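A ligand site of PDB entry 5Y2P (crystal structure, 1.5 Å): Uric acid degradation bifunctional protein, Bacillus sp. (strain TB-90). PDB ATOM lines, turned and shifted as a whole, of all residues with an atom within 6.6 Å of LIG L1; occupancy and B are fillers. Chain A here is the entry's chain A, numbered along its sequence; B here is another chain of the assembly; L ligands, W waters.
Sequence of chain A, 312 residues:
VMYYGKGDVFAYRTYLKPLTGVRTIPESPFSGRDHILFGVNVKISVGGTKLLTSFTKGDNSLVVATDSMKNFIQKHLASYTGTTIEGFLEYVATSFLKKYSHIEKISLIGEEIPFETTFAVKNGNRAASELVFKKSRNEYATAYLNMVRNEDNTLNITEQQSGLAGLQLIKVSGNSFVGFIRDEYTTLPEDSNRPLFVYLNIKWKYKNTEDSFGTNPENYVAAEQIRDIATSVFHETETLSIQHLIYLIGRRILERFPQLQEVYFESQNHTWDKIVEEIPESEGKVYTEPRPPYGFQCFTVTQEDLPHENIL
Phe 177 touches LIG L1.
Leu 188 touches LIG L1 (CD2 to N4, 3.6 Å).
CA of Ser 241 touches O1 of LIG L1 (3.3 Å).
Gln 297 touches LIG L1 (NE2 to N1, 3.9 Å).
Tyr 4 of chain B touches LIG L1 (CE2 to O2, 3.7 Å).
Val 63 of chain B touches LIG L1 (CG1 to O2, 3.9 Å).
Ala 65 of chain B touches LIG L1.
N of Asp 67 of chain B touches N4 of LIG L1, 3.9 Å away.
Of the 25 residues printed, 13 come within 4 Å of LIG L1.
The nearest printed residue that does not touch LIG L1 is Val 64 of chain B (4.9 Å).
Water W2 bridges N5 of LIG L1 and NH1 of Arg 194.
Water W1 lies within hydrogen-bond range of the side-chain amino group of Lys 6 of chain B (2.8 Å), the side-chain hydroxyl of Thr 66 of chain B (3.3 Å), an oxygen (O1) of LG2 L2 (3.3 Å) and a nitrogen (N4) of LIG L1 (3.3 Å).
An oxygen (O1) of LG2 L2 lies close to a nitrogen (N5) of LIG L1, at 3.4 Å.
An oxygen (O1) of LIG L1 lies within hydrogen-bond range of the guanidinium group (NH2) of Arg 194 (2.7 Å).
The backbone NH of Ile 242 is in hydrogen-bond range of an oxygen (O1) of LIG L1 (2.8 Å).
The backbone NH (N) of Thr 66 of chain B lies within hydrogen-bond range of a nitrogen (N3) of LIG L1 (2.9 Å).
The side-chain hydroxyl (OG1) of Thr 66 of chain B lies within hydrogen-bond range of a nitrogen (N3) of LIG L1 (3.3 Å).
A nitrogen (N1) of LIG L1 lies within hydrogen-bond range of the side-chain amide oxygen of Gln 243 (2.9 Å).
A nitrogen (N2) of LIG L1 lies close to the side-chain amide nitrogen of Asn 269, 3.5 Å away.
The side-chain hydroxyl (OG1) of Thr 66 of chain B is in hydrogen-bond range of an oxygen (O1) of LG2 L2.
The side-chain amide nitrogen of Asn 269 lies within hydrogen-bond range of an oxygen (O1) of LG2 L2 (3.1 Å).
The side-chain amide nitrogen (NE2) of Gln 297 is in hydrogen-bond range of an oxygen (O2) of LG2 L2 (3.3 Å).
The side-chain amino group of Lys 6 of chain B lies within hydrogen-bond range of the side-chain hydroxyl of Thr 66 of chain B, 3.1 Å away.
The side-chain hydroxyl (OG) of Ser 241 lies close to the backbone NH (N) of Gln 243, at 3.3 Å.
The backbone NH (N) of Asn 269 lies within hydrogen-bond range of the backbone carbonyl oxygen (O) of Gly 295.
The side-chain hydroxyl (OH) of Tyr 4 of chain B lies within hydrogen-bond range of the backbone carbonyl oxygen (O) of Val 64 of chain B (2.7 Å).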
ATOM      1  N   SER A 176      25.238  18.762  18.876  1.00  0.00           N
ATOM      2  CA  SER A 176      24.109  19.673  18.740  1.00  0.00           C
ATOM      3  C   SER A 176      22.910  19.158  19.525  1.00  0.00           C
ATOM      4  O   SER A 176      22.772  17.961  19.820  1.00  0.00           O
ATOM      5  CB  SER A 176      23.663  19.845  17.295  1.00  0.00           C
ATOM      6  OG  SER A 176      23.029  18.701  16.820  1.00  0.00           O
ATOM      7  N   PHE A 177      22.025  20.091  19.868  1.00  0.00           N
ATOM      8  CA  PHE A 177      20.709  19.739  20.394  1.00  0.00           C
ATOM      9  C   PHE A 177      19.733  20.746  19.808  1.00  0.00           C
ATOM     10  O   PHE A 177      19.580  21.851  20.318  1.00  0.00           O
ATOM     11  CB  PHE A 177      20.635  19.664  21.914  1.00  0.00           C
ATOM     12  CG  PHE A 177      19.331  19.077  22.404  1.00  0.00           C
ATOM     13  CD1 PHE A 177      18.966  17.788  21.999  1.00  0.00           C
ATOM     14  CD2 PHE A 177      18.468  19.797  23.222  1.00  0.00           C
ATOM     15  CE1 PHE A 177      17.762  17.249  22.397  1.00  0.00           C
ATOM     16  CE2 PHE A 177      17.271  19.256  23.613  1.00  0.00           C
ATOM     17  CZ  PHE A 177      16.918  17.978  23.202  1.00  0.00           C
ATOM     18  N   PHE A 180      13.922  20.048  18.995  1.00  0.00           N
ATOM     19  CA  PHE A 180      12.995  19.607  20.022  1.00  0.00           C
ATOM     20  C   PHE A 180      11.757  20.512  20.085  1.00  0.00           C
ATOM     21  O   PHE A 180      11.679  21.572  19.453  1.00  0.00           O
ATOM     22  CB  PHE A 180      13.736  19.523  21.363  1.00  0.00           C
ATOM     23  CG  PHE A 180      14.471  20.800  21.731  1.00  0.00           C
ATOM     24  CD1 PHE A 180      13.819  21.774  22.462  1.00  0.00           C
ATOM     25  CD2 PHE A 180      15.791  21.008  21.364  1.00  0.00           C
ATOM     26  CE1 PHE A 180      14.462  22.962  22.801  1.00  0.00           C
ATOM     27  CE2 PHE A 180      16.449  22.198  21.701  1.00  0.00           C
ATOM     28  CZ  PHE A 180      15.780  23.172  22.416  1.00  0.00           C
ATOM     29  N   LEU A 188      14.580  26.654  26.506  1.00  0.00           N
ATOM     30  CA  LEU A 188      15.936  26.269  26.111  1.00  0.00           C
ATOM     31  C   LEU A 188      16.211  26.684  24.668  1.00  0.00           C
ATOM     32  O   LEU A 188      15.481  26.269  23.763  1.00  0.00           O
ATOM     33  CB  LEU A 188      16.064  24.745  26.221  1.00  0.00           C
ATOM     34  CG  LEU A 188      17.421  24.130  25.910  1.00  0.00           C
ATOM     35  CD1 LEU A 188      18.434  24.599  26.929  1.00  0.00           C
ATOM     36  CD2 LEU A 188      17.393  22.606  25.879  1.00  0.00           C
ATOM     37  N   ARG A 194      27.425  22.512  21.253  1.00  0.00           N
ATOM     38  CA  ARG A 194      27.494  22.565  22.708  1.00  0.00           C
ATOM     39  C   ARG A 194      28.612  21.673  23.204  1.00  0.00           C
ATOM     40  O   ARG A 194      28.978  20.695  22.539  1.00  0.00           O
ATOM     41  CB  ARG A 194      26.171  22.145  23.366  1.00  0.00           C
ATOM     42  CG  ARG A 194      25.785  20.710  23.081  1.00  0.00           C
ATOM     43  CD  ARG A 194      24.453  20.370  23.744  1.00  0.00           C
ATOM     44  NE  ARG A 194      24.079  18.974  23.486  1.00  0.00           N
ATOM     45  CZ  ARG A 194      23.077  18.355  24.097  1.00  0.00           C
ATOM     46  NH1 ARG A 194      22.352  19.002  24.991  1.00  0.00           N
ATOM     47  NH2 ARG A 194      22.797  17.092  23.797  1.00  0.00           N
ATOM     48  N   LEU A 196      28.946  19.057  25.156  1.00  0.00           N
ATOM     49  CA  LEU A 196      28.144  18.044  25.844  1.00  0.00           C
ATOM     50  C   LEU A 196      28.947  17.324  26.939  1.00  0.00           C
ATOM     51  O   LEU A 196      30.008  16.764  26.679  1.00  0.00           O
ATOM     52  CB  LEU A 196      27.638  17.021  24.843  1.00  0.00           C
ATOM     53  CG  LEU A 196      26.835  15.862  25.409  1.00  0.00           C
ATOM     54  CD1 LEU A 196      25.648  16.361  26.220  1.00  0.00           C
ATOM     55  CD2 LEU A 196      26.340  14.957  24.304  1.00  0.00           C
ATOM     56  N   LEU A 240      23.662  14.274  18.267  1.00  0.00           N
ATOM     57  CA  LEU A 240      22.414  15.009  18.077  1.00  0.00           C
ATOM     58  C   LEU A 240      21.585  15.111  19.339  1.00  0.00           C
ATOM     59  O   LEU A 240      20.587  15.845  19.367  1.00  0.00           O
ATOM     60  CB  LEU A 240      21.598  14.330  16.964  1.00  0.00           C
ATOM     61  CG  LEU A 240      22.266  14.322  15.568  1.00  0.00           C
ATOM     62  CD1 LEU A 240      21.446  13.487  14.595  1.00  0.00           C
ATOM     63  CD2 LEU A 240      22.451  15.748  15.020  1.00  0.00           C
ATOM     64  N   SER A 241      21.971  14.368  20.379  1.00  0.00           N
ATOM     65  CA  SER A 241      21.373  14.327  21.703  1.00  0.00           C
ATOM     66  C   SER A 241      22.163  13.266  22.444  1.00  0.00           C
ATOM     67  O   SER A 241      22.930  12.510  21.848  1.00  0.00           O
ATOM     68  CB  SER A 241      19.903  13.926  21.672  1.00  0.00           C
ATOM     69  OG  SER A 241      19.772  12.613  21.145  1.00  0.00           O
ATOM     70  N   ILE A 242      21.971  13.228  23.747  1.00  0.00           N
ATOM     71  CA  ILE A 242      22.500  12.108  24.527  1.00  0.00           C
ATOM     72  C   ILE A 242      21.866  10.809  24.063  1.00  0.00           C
ATOM     73  O   ILE A 242      22.524   9.764  23.972  1.00  0.00           O
ATOM     74  CB  ILE A 242      22.321  12.351  26.032  1.00  0.00           C
ATOM     75  CG1 ILE A 242      23.169  13.520  26.462  1.00  0.00           C
ATOM     76  CG2 ILE A 242      22.776  11.133  26.802  1.00  0.00           C
ATOM     77  CD1 ILE A 242      22.816  14.047  27.868  1.00  0.00           C
ATOM     78  N   GLN A 243      20.547  10.834  23.855  1.00  0.00           N
ATOM     79  CA  GLN A 243      19.804   9.667  23.396  1.00  0.00           C
ATOM     80  C   GLN A 243      20.464   9.048  22.168  1.00  0.00           C
ATOM     81  O   GLN A 243      20.660   7.832  22.101  1.00  0.00           O
ATOM     82  CB  GLN A 243      18.376  10.106  23.033  1.00  0.00           C
ATOM     83  CG  GLN A 243      17.447  10.496  24.223  1.00  0.00           C
ATOM     84  CD  GLN A 243      17.498  11.978  24.597  1.00  0.00           C
ATOM     85  OE1 GLN A 243      18.551  12.616  24.609  1.00  0.00           O
ATOM     86  NE2 GLN A 243      16.343  12.524  24.972  1.00  0.00           N
ATOM     87  N   ASN A 269      22.870  14.435  31.914  1.00  0.00           N
ATOM     88  CA  ASN A 269      23.374  15.636  31.270  1.00  0.00           C
ATOM     89  C   ASN A 269      23.828  16.649  32.310  1.00  0.00           C
ATOM     90  O   ASN A 269      23.029  17.053  33.160  1.00  0.00           O
ATOM     91  CB  ASN A 269      22.272  16.260  30.436  1.00  0.00           C
ATOM     92  CG  ASN A 269      22.772  17.293  29.456  1.00  0.00           C
ATOM     93  OD1 ASN A 269      23.863  17.829  29.586  1.00  0.00           O
ATOM     94  ND2 ASN A 269      21.963  17.561  28.460  1.00  0.00           N
ATOM     95  N   GLY A 295      19.240  16.476  33.283  1.00  0.00           N
ATOM     96  CA  GLY A 295      18.542  15.524  32.458  1.00  0.00           C
ATOM     97  C   GLY A 295      19.134  14.152  32.593  1.00  0.00           C
ATOM     98  O   GLY A 295      20.294  13.955  32.938  1.00  0.00           O
ATOM     99  N   PHE A 296      18.305  13.151  32.280  1.00  0.00           N
ATOM    100  CA  PHE A 296      18.798  11.785  32.286  1.00  0.00           C
ATOM    101  C   PHE A 296      18.042  10.965  31.255  1.00  0.00           C
ATOM    102  O   PHE A 296      16.952  11.324  30.804  1.00  0.00           O
ATOM    103  CB  PHE A 296      18.690  11.124  33.664  1.00  0.00           C
ATOM    104  CG  PHE A 296      17.286  10.958  34.180  1.00  0.00           C
ATOM    105  CD1 PHE A 296      16.525   9.878  33.803  1.00  0.00           C
ATOM    106  CD2 PHE A 296      16.757  11.867  35.072  1.00  0.00           C
ATOM    107  CE1 PHE A 296      15.246   9.720  34.295  1.00  0.00           C
ATOM    108  CE2 PHE A 296      15.487  11.705  35.573  1.00  0.00           C
ATOM    109  CZ  PHE A 296      14.745  10.648  35.191  1.00  0.00           C
ATOM    110  N   GLN A 297      18.679   9.858  30.860  1.00  0.00           N
ATOM    111  CA  GLN A 297      18.148   8.922  29.861  1.00  0.00           C
ATOM    112  C   GLN A 297      18.464   7.499  30.336  1.00  0.00           C
ATOM    113  O   GLN A 297      19.482   7.256  31.007  1.00  0.00           O
ATOM    114  CB  GLN A 297      18.803   9.119  28.507  1.00  0.00           C
ATOM    115  CG  GLN A 297      18.647  10.445  27.862  1.00  0.00           C
ATOM    116  CD  GLN A 297      19.430  11.619  28.517  1.00  0.00           C
ATOM    117  OE1 GLN A 297      20.465  11.441  29.153  1.00  0.00           O
ATOM    118  NE2 GLN A 297      18.916  12.831  28.314  1.00  0.00           N
ATOM    119  N   TYR B   4      13.301   8.855  29.612  1.00  0.00           N
ATOM    120  CA  TYR B   4      14.185   9.991  29.859  1.00  0.00           C
ATOM    121  C   TYR B   4      13.439  10.972  30.742  1.00  0.00           C
ATOM    122  O   TYR B   4      12.213  10.892  30.909  1.00  0.00           O
ATOM    123  CB  TYR B   4      14.705  10.600  28.528  1.00  0.00           C
ATOM    124  CG  TYR B   4      13.754  11.557  27.840  1.00  0.00           C
ATOM    125  CD1 TYR B   4      12.548  11.135  27.339  1.00  0.00           C
ATOM    126  CD2 TYR B   4      14.110  12.867  27.663  1.00  0.00           C
ATOM    127  CE1 TYR B   4      11.677  12.036  26.735  1.00  0.00           C
ATOM    128  CE2 TYR B   4      13.289  13.755  27.041  1.00  0.00           C
ATOM    129  CZ  TYR B   4      12.061  13.324  26.593  1.00  0.00           C
ATOM    130  OH  TYR B   4      11.183  14.173  26.002  1.00  0.00           O
ATOM    131  N   GLY B   5      14.179  11.916  31.321  1.00  0.00           N
ATOM    132  CA  GLY B   5      13.552  12.835  32.243  1.00  0.00           C
ATOM    133  C   GLY B   5      14.511  13.801  32.900  1.00  0.00           C
ATOM    134  O   GLY B   5      15.564  14.116  32.347  1.00  0.00           O
ATOM    135  N   LYS B   6      14.091  14.329  34.050  1.00  0.00           N
ATOM    136  CA  LYS B   6      14.830  15.372  34.752  1.00  0.00           C
ATOM    137  C   LYS B   6      14.835  15.041  36.239  1.00  0.00           C
ATOM    138  O   LYS B   6      13.782  14.733  36.805  1.00  0.00           O
ATOM    139  CB  LYS B   6      14.173  16.747  34.538  1.00  0.00           C
ATOM    140  CG  LYS B   6      15.065  17.936  34.860  1.00  0.00           C
ATOM    141  CD  LYS B   6      16.029  18.160  33.716  1.00  0.00           C
ATOM    142  CE  LYS B   6      16.729  19.489  33.784  1.00  0.00           C
ATOM    143  NZ  LYS B   6      17.527  19.654  32.539  1.00  0.00           N
ATOM    144  N   ASN B  60      14.670  14.709  17.098  1.00  0.00           N
ATOM    145  CA  ASN B  60      14.163  15.340  18.300  1.00  0.00           C
ATOM    146  C   ASN B  60      12.755  15.894  18.147  1.00  0.00           C
ATOM    147  O   ASN B  60      12.266  16.567  19.076  1.00  0.00           O
ATOM    148  CB  ASN B  60      15.135  16.431  18.736  1.00  0.00           C
ATOM    149  CG  ASN B  60      16.441  15.861  19.214  1.00  0.00           C
ATOM    150  OD1 ASN B  60      16.440  14.861  19.921  1.00  0.00           O
ATOM    151  ND2 ASN B  60      17.557  16.483  18.831  1.00  0.00           N
ATOM    152  N   VAL B  63      10.641  15.179  21.074  1.00  0.00           N
ATOM    153  CA  VAL B  63      11.327  15.316  22.354  1.00  0.00           C
ATOM    154  C   VAL B  63      10.854  16.595  23.038  1.00  0.00           C
ATOM    155  O   VAL B  63      11.061  17.707  22.538  1.00  0.00           O
ATOM    156  CB  VAL B  63      12.860  15.294  22.193  1.00  0.00           C
ATOM    157  CG1 VAL B  63      13.548  15.574  23.525  1.00  0.00           C
ATOM    158  CG2 VAL B  63      13.298  13.944  21.646  1.00  0.00           C
ATOM    159  N   VAL B  64      10.198  16.429  24.190  1.00  0.00           N
ATOM    160  CA  VAL B  64      10.058  17.496  25.162  1.00  0.00           C
ATOM    161  C   VAL B  64      11.410  17.631  25.853  1.00  0.00           C
ATOM    162  O   VAL B  64      11.889  16.684  26.478  1.00  0.00           O
ATOM    163  CB  VAL B  64       8.978  17.129  26.186  1.00  0.00           C
ATOM    164  CG1 VAL B  64       8.867  18.223  27.264  1.00  0.00           C
ATOM    165  CG2 VAL B  64       7.636  16.864  25.508  1.00  0.00           C
ATOM    166  N   ALA B  65      12.023  18.779  25.740  1.00  0.00           N
ATOM    167  CA  ALA B  65      13.318  18.975  26.368  1.00  0.00           C
ATOM    168  C   ALA B  65      13.214  18.722  27.865  1.00  0.00           C
ATOM    169  O   ALA B  65      12.216  19.066  28.496  1.00  0.00           O
ATOM    170  CB  ALA B  65      13.877  20.367  26.085  1.00  0.00           C
ATOM    171  N   THR B  66      14.234  18.113  28.452  1.00  0.00           N
ATOM    172  CA  THR B  66      14.189  17.923  29.897  1.00  0.00           C
ATOM    173  C   THR B  66      14.174  19.245  30.640  1.00  0.00           C
ATOM    174  O   THR B  66      13.546  19.352  31.693  1.00  0.00           O
ATOM    175  CB  THR B  66      15.345  17.047  30.367  1.00  0.00           C
ATOM    176  OG1 THR B  66      16.562  17.761  30.252  1.00  0.00           O
ATOM    177  CG2 THR B  66      15.402  15.756  29.582  1.00  0.00           C
ATOM    178  N   ASP B  67      14.798  20.282  30.056  1.00  0.00           N
ATOM    179  CA  ASP B  67      14.672  21.619  30.626  1.00  0.00           C
ATOM    180  C   ASP B  67      13.219  22.096  30.644  1.00  0.00           C
ATOM    181  O   ASP B  67      12.799  22.793  31.574  1.00  0.00           O
ATOM    182  CB  ASP B  67      15.532  22.571  29.783  1.00  0.00           C
ATOM    183  CG  ASP B  67      15.582  23.952  30.380  1.00  0.00           C
ATOM    184  OD1 ASP B  67      16.375  24.167  31.318  1.00  0.00           O
ATOM    185  OD2 ASP B  67      14.805  24.833  29.921  1.00  0.00           O
ATOM    186  N   SER B  68      12.450  21.769  29.597  1.00  0.00           N
ATOM    187  CA  SER B  68      11.029  22.127  29.574  1.00  0.00           C
ATOM    188  C   SER B  68      10.237  21.370  30.631  1.00  0.00           C
ATOM    189  O   SER B  68       9.291  21.934  31.206  1.00  0.00           O
ATOM    190  CB  SER B  68      10.448  21.874  28.193  1.00  0.00           C
ATOM    191  OG  SER B  68      11.238  22.556  27.233  1.00  0.00           O
ATOM    192  N   MET B  69      10.608  20.113  30.927  1.00  0.00           N
ATOM    193  CA  MET B  69       9.998  19.373  32.041  1.00  0.00           C
ATOM    194  C   MET B  69      10.215  20.091  33.360  1.00  0.00           C
ATOM    195  O   MET B  69       9.300  20.151  34.205  1.00  0.00           O
ATOM    196  CB  MET B  69      10.574  17.952  32.090  1.00  0.00           C
ATOM    197  CG  MET B  69      10.354  17.146  30.844  1.00  0.00           C
ATOM    198  SD  MET B  69      11.066  15.521  31.087  1.00  0.00           S
ATOM    199  CE  MET B  69      10.917  14.860  29.423  1.00  0.00           C
HETATM  200  N1  LIG L   1      18.603  15.404  25.413  1.00  0.00           N
HETATM  201  C1  LIG L   1      19.801  16.082  25.279  1.00  0.00           C
HETATM  202  O1  LIG L   1      20.767  15.513  24.753  1.00  0.00           O
HETATM  203  N2  LIG L   1      19.851  17.344  25.715  1.00  0.00           N
HETATM  204  C2  LIG L   1      18.774  17.905  26.263  1.00  0.00           C
HETATM  205  C3  LIG L   1      17.595  17.229  26.372  1.00  0.00           C
HETATM  206  C4  LIG L   1      17.495  15.918  25.947  1.00  0.00           C
HETATM  207  O2  LIG L   1      16.509  15.236  26.046  1.00  0.00           O
HETATM  208  N3  LIG L   1      16.705  18.060  26.979  1.00  0.00           N
HETATM  209  N4  LIG L   1      17.315  19.215  27.223  1.00  0.00           N
HETATM  210  N5  LIG L   1      18.583  19.136  26.763  1.00  0.00           N
HETATM  211  O1  LG2 L   2      19.099  17.011  29.385  1.00  0.00           O
HETATM  212  O2  LG2 L   2      19.064  16.006  29.059  1.00  0.00           O
HETATM  213  O   HOH W   1      18.686  20.234  30.081  1.00  0.00           O
HETATM  214  O   HOH W   2      20.673  21.057  27.163  1.00  0.00           O
